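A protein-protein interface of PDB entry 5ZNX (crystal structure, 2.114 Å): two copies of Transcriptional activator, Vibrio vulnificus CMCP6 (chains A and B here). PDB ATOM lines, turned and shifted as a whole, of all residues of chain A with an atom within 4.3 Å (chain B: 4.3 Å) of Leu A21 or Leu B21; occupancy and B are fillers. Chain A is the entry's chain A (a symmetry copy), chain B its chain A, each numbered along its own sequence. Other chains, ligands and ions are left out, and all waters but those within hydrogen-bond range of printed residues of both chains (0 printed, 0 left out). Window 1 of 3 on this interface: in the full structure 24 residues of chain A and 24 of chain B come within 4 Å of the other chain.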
ATOM      1  N   ALA A  17       4.467 -22.058  -0.622  1.00  0.00           N
ATOM      2  CA  ALA A  17       5.171 -23.099   0.116  1.00  0.00           C
ATOM      3  C   ALA A  17       4.926 -22.975   1.615  1.00  0.00           C
ATOM      4  O   ALA A  17       4.768 -23.990   2.306  1.00  0.00           O
ATOM      5  CB  ALA A  17       6.667 -23.041  -0.192  1.00  0.00           C
ATOM      6  N   VAL A  18       4.885 -21.744   2.137  1.00  0.00           N
ATOM      7  CA  VAL A  18       4.665 -21.551   3.571  1.00  0.00           C
ATOM      8  C   VAL A  18       3.286 -22.061   3.977  1.00  0.00           C
ATOM      9  O   VAL A  18       3.118 -22.641   5.059  1.00  0.00           O
ATOM     10  CB  VAL A  18       4.879 -20.075   3.956  1.00  0.00           C
ATOM     11  CG1 VAL A  18       4.149 -19.738   5.247  1.00  0.00           C
ATOM     12  CG2 VAL A  18       6.365 -19.800   4.120  1.00  0.00           C
ATOM     13  N   VAL A  19       2.278 -21.870   3.117  1.00  0.00           N
ATOM     14  CA  VAL A  19       0.945 -22.377   3.430  1.00  0.00           C
ATOM     15  C   VAL A  19       1.010 -23.883   3.657  1.00  0.00           C
ATOM     16  O   VAL A  19       0.435 -24.414   4.614  1.00  0.00           O
ATOM     17  CB  VAL A  19      -0.046 -22.013   2.308  1.00  0.00           C
ATOM     18  CG1 VAL A  19      -1.280 -22.894   2.380  1.00  0.00           C
ATOM     19  CG2 VAL A  19      -0.430 -20.542   2.392  1.00  0.00           C
ATOM     20  N   LEU A  20       1.738 -24.589   2.790  1.00  0.00           N
ATOM     21  CA  LEU A  20       1.882 -26.032   2.928  1.00  0.00           C
ATOM     22  C   LEU A  20       2.703 -26.389   4.161  1.00  0.00           C
ATOM     23  O   LEU A  20       2.359 -27.327   4.892  1.00  0.00           O
ATOM     24  CB  LEU A  20       2.519 -26.603   1.659  1.00  0.00           C
ATOM     25  CG  LEU A  20       3.121 -28.006   1.668  1.00  0.00           C
ATOM     26  CD1 LEU A  20       2.057 -29.046   1.952  1.00  0.00           C
ATOM     27  CD2 LEU A  20       3.814 -28.293   0.341  1.00  0.00           C
ATOM     28  N   LEU A  21       3.786 -25.648   4.417  1.00  0.00           N
ATOM     29  CA  LEU A  21       4.624 -25.934   5.576  1.00  0.00           C
ATOM     30  C   LEU A  21       3.879 -25.671   6.879  1.00  0.00           C
ATOM     31  O   LEU A  21       3.983 -26.463   7.825  1.00  0.00           O
ATOM     32  CB  LEU A  21       5.910 -25.111   5.507  1.00  0.00           C
ATOM     33  CG  LEU A  21       6.908 -25.582   4.445  1.00  0.00           C
ATOM     34  CD1 LEU A  21       7.898 -24.473   4.097  1.00  0.00           C
ATOM     35  CD2 LEU A  21       7.636 -26.829   4.914  1.00  0.00           C
ATOM     36  N   LYS A  22       3.120 -24.571   6.948  1.00  0.00           N
ATOM     37  CA  LYS A  22       2.359 -24.281   8.162  1.00  0.00           C
ATOM     38  C   LYS A  22       1.325 -25.364   8.432  1.00  0.00           C
ATOM     39  O   LYS A  22       1.048 -25.683   9.591  1.00  0.00           O
ATOM     40  CB  LYS A  22       1.667 -22.920   8.054  1.00  0.00           C
ATOM     41  CG  LYS A  22       2.504 -21.736   8.516  1.00  0.00           C
ATOM     42  CD  LYS A  22       1.744 -20.423   8.334  1.00  0.00           C
ATOM     43  CE  LYS A  22       2.602 -19.219   8.701  1.00  0.00           C
ATOM     44  NZ  LYS A  22       1.969 -17.928   8.294  1.00  0.00           N
ATOM     45  N   ALA A  23       0.746 -25.942   7.377  1.00  0.00           N
ATOM     46  CA  ALA A  23      -0.243 -26.992   7.579  1.00  0.00           C
ATOM     47  C   ALA A  23       0.398 -28.258   8.133  1.00  0.00           C
ATOM     48  O   ALA A  23      -0.247 -28.998   8.883  1.00  0.00           O
ATOM     49  CB  ALA A  23      -0.981 -27.284   6.274  1.00  0.00           C
ATOM     50  N   MET A  24       1.659 -28.519   7.785  1.00  0.00           N
ATOM     51  CA  MET A  24       2.354 -29.703   8.273  1.00  0.00           C
ATOM     52  C   MET A  24       3.070 -29.475   9.596  1.00  0.00           C
ATOM     53  O   MET A  24       3.417 -30.451  10.267  1.00  0.00           O
ATOM     54  CB  MET A  24       3.391 -30.185   7.251  1.00  0.00           C
ATOM     55  CG  MET A  24       2.869 -30.393   5.839  1.00  0.00           C
ATOM     56  SD  MET A  24       4.232 -30.624   4.666  1.00  0.00           S
ATOM     57  CE  MET A  24       4.890 -32.175   5.234  1.00  0.00           C
ATOM     58  N   ALA A  25       3.303 -28.217   9.980  1.00  0.00           N
ATOM     59  CA  ALA A  25       4.015 -27.886  11.217  1.00  0.00           C
ATOM     60  C   ALA A  25       3.125 -28.048  12.454  1.00  0.00           C
ATOM     61  O   ALA A  25       2.902 -27.118  13.226  1.00  0.00           O
ATOM     62  CB  ALA A  25       4.574 -26.472  11.124  1.00  0.00           C
ATOM     63  N   LEU A  30       0.700 -33.559  11.094  1.00  0.00           N
ATOM     64  CA  LEU A  30       1.746 -34.317  10.418  1.00  0.00           C
ATOM     65  C   LEU A  30       1.508 -35.818  10.535  1.00  0.00           C
ATOM     66  O   LEU A  30       1.746 -36.565   9.579  1.00  0.00           O
ATOM     67  CB  LEU A  30       3.120 -33.959  10.985  1.00  0.00           C
ATOM     68  CG  LEU A  30       4.269 -34.639  10.237  1.00  0.00           C
ATOM     69  CD1 LEU A  30       4.284 -34.166   8.787  1.00  0.00           C
ATOM     70  CD2 LEU A  30       5.608 -34.373  10.912  1.00  0.00           C
ATOM     71  N   ALA B  17      10.445 -33.619  13.814  1.00  0.00           N
ATOM     72  CA  ALA B  17      10.117 -33.124  12.483  1.00  0.00           C
ATOM     73  C   ALA B  17       9.364 -31.801  12.556  1.00  0.00           C
ATOM     74  O   ALA B  17       9.603 -30.903  11.738  1.00  0.00           O
ATOM     75  CB  ALA B  17       9.300 -34.167  11.721  1.00  0.00           C
ATOM     76  N   VAL B  18       8.457 -31.657  13.528  1.00  0.00           N
ATOM     77  CA  VAL B  18       7.690 -30.417  13.651  1.00  0.00           C
ATOM     78  C   VAL B  18       8.611 -29.243  13.966  1.00  0.00           C
ATOM     79  O   VAL B  18       8.409 -28.127  13.466  1.00  0.00           O
ATOM     80  CB  VAL B  18       6.568 -30.577  14.695  1.00  0.00           C
ATOM     81  CG1 VAL B  18       6.134 -29.224  15.239  1.00  0.00           C
ATOM     82  CG2 VAL B  18       5.379 -31.282  14.064  1.00  0.00           C
ATOM     83  N   VAL B  19       9.643 -29.470  14.787  1.00  0.00           N
ATOM     84  CA  VAL B  19      10.587 -28.397  15.089  1.00  0.00           C
ATOM     85  C   VAL B  19      11.199 -27.873  13.795  1.00  0.00           C
ATOM     86  O   VAL B  19      11.304 -26.660  13.578  1.00  0.00           O
ATOM     87  CB  VAL B  19      11.666 -28.890  16.071  1.00  0.00           C
ATOM     88  CG1 VAL B  19      12.876 -27.973  16.038  1.00  0.00           C
ATOM     89  CG2 VAL B  19      11.102 -28.984  17.482  1.00  0.00           C
ATOM     90  N   LEU B  20      11.586 -28.786  12.903  1.00  0.00           N
ATOM     91  CA  LEU B  20      12.166 -28.392  11.625  1.00  0.00           C
ATOM     92  C   LEU B  20      11.128 -27.721  10.733  1.00  0.00           C
ATOM     93  O   LEU B  20      11.424 -26.713  10.079  1.00  0.00           O
ATOM     94  CB  LEU B  20      12.769 -29.620  10.940  1.00  0.00           C
ATOM     95  CG  LEU B  20      13.105 -29.579   9.451  1.00  0.00           C
ATOM     96  CD1 LEU B  20      14.169 -28.537   9.169  1.00  0.00           C
ATOM     97  CD2 LEU B  20      13.558 -30.954   8.973  1.00  0.00           C
ATOM     98  N   LEU B  21       9.904 -28.257  10.700  1.00  0.00           N
ATOM     99  CA  LEU B  21       8.860 -27.673   9.865  1.00  0.00           C
ATOM    100  C   LEU B  21       8.467 -26.285  10.355  1.00  0.00           C
ATOM    101  O   LEU B  21       8.278 -25.370   9.544  1.00  0.00           O
ATOM    102  CB  LEU B  21       7.646 -28.601   9.821  1.00  0.00           C
ATOM    103  CG  LEU B  21       7.849 -29.871   8.991  1.00  0.00           C
ATOM    104  CD1 LEU B  21       6.834 -30.944   9.378  1.00  0.00           C
ATOM    105  CD2 LEU B  21       7.764 -29.558   7.508  1.00  0.00           C
ATOM    106  N   LYS B  22       8.345 -26.105  11.676  1.00  0.00           N
ATOM    107  CA  LYS B  22       7.998 -24.789  12.207  1.00  0.00           C
ATOM    108  C   LYS B  22       9.072 -23.764  11.875  1.00  0.00           C
ATOM    109  O   LYS B  22       8.762 -22.593  11.641  1.00  0.00           O
ATOM    110  CB  LYS B  22       7.797 -24.854  13.724  1.00  0.00           C
ATOM    111  CG  LYS B  22       6.384 -25.203  14.169  1.00  0.00           C
ATOM    112  CD  LYS B  22       6.293 -25.281  15.692  1.00  0.00           C
ATOM    113  CE  LYS B  22       4.910 -25.723  16.152  1.00  0.00           C
ATOM    114  NZ  LYS B  22       4.876 -26.045  17.611  1.00  0.00           N
ATOM    115  N   ALA B  23      10.339 -24.183  11.846  1.00  0.00           N
ATOM    116  CA  ALA B  23      11.405 -23.246  11.522  1.00  0.00           C
ATOM    117  C   ALA B  23      11.338 -22.813  10.063  1.00  0.00           C
ATOM    118  O   ALA B  23      11.714 -21.682   9.737  1.00  0.00           O
ATOM    119  CB  ALA B  23      12.767 -23.858  11.844  1.00  0.00           C
ATOM    120  N   MET B  24      10.861 -23.688   9.176  1.00  0.00           N
ATOM    121  CA  MET B  24      10.754 -23.357   7.761  1.00  0.00           C
ATOM    122  C   MET B  24       9.430 -22.703   7.397  1.00  0.00           C
ATOM    123  O   MET B  24       9.335 -22.093   6.328  1.00  0.00           O
ATOM    124  CB  MET B  24      10.914 -24.614   6.896  1.00  0.00           C
ATOM    125  CG  MET B  24      12.155 -25.446   7.177  1.00  0.00           C
ATOM    126  SD  MET B  24      12.060 -27.057   6.350  1.00  0.00           S
ATOM    127  CE  MET B  24      12.123 -26.550   4.646  1.00  0.00           C
ATOM    128  N   ALA B  25       8.410 -22.820   8.252  1.00  0.00           N
ATOM    129  CA  ALA B  25       7.083 -22.259   7.984  1.00  0.00           C
ATOM    130  C   ALA B  25       7.041 -20.745   8.217  1.00  0.00           C
ATOM    131  O   ALA B  25       6.266 -20.227   9.017  1.00  0.00           O
ATOM    132  CB  ALA B  25       6.043 -22.975   8.837  1.00  0.00           C
ATOM    133  N   LEU B  30      12.227 -19.239   5.226  1.00  0.00           N
ATOM    134  CA  LEU B  30      12.330 -20.148   4.090  1.00  0.00           C
ATOM    135  C   LEU B  30      13.196 -19.558   2.984  1.00  0.00           C
ATOM    136  O   LEU B  30      13.970 -20.279   2.344  1.00  0.00           O
ATOM    137  CB  LEU B  30      10.942 -20.486   3.546  1.00  0.00           C
ATOM    138  CG  LEU B  30      10.979 -21.527   2.425  1.00  0.00           C
ATOM    139  CD1 LEU B  30      11.542 -22.837   2.964  1.00  0.00           C
ATOM    140  CD2 LEU B  30       9.601 -21.735   1.812  1.00  0.00           C
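Among the printed residues, pairs that only touch across the chains: Ala A17 with Leu B30, Leu A21 with Leu B21, Leu A21 with Met B24, Leu A21 with Ala B25, Leu A21 with Leu B30, Lys A22 with Ala B25, Met A24 with Leu B21, Ala A25 with Leu B21, Ala A25 with Lys B22, Leu A30 with Ala B17 and Leu A30 with Leu B21.
Of the printed residues of chain B, Lys A22 touches Ala B25.
Of the printed residues of chain B, Ala A25 touches Leu B21 (3.96 Å) and Lys B22 (3.8 Å).
Leu B21 touches four residues of chain A.
The nearest printed residue of chain A that does not touch Leu B21 is Lys A22 (5.8 Å).
The nearest printed residue of chain B that does not touch Ala A17 is Ala B25 (6.4 Å).
Printed residues of chain B that touch a printed residue of chain A: Ala B17, Leu B21, Lys B22, Met B24, Ala B25 and Leu B30.
Hydrophobic or aromatic side chains of chain B within 4 Å of the printed part of chain A: Ala B17, Leu B21, Ala B25 and Leu B30.
Printed residues of chain A that touch a printed residue of chain B: Ala A17, Leu A21, Lys A22, Met A24, Ala A25 and Leu A30.
Hydrophobic or aromatic side chains of chain A that line the printed part of chain B: Ala A17, Leu A21, Ala A25 and Leu A30.
Along chain A the printed residues that touch a printed residue of chain B span positions 17 to 30.
Ala A17 touches Leu B30, and with the chains exchanged Leu A30 touches Ala B17.
Leu A21 touches Met B24, and with the chains exchanged Met A24 touches Leu B21.
Leu A21 touches Ala B25, and with the chains exchanged Ala A25 touches Leu B21.
Lys A22 touches Ala B25, and with the chains exchanged Ala A25 touches Lys B22.
Positions printed for both chains: 17, 18, 19, 20, 21, 22, 23, 24, 25 and 30.
Of the 11 pairs that touch across the chains among the printed residues, 11 have their exchanged pair printed and touching as well.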
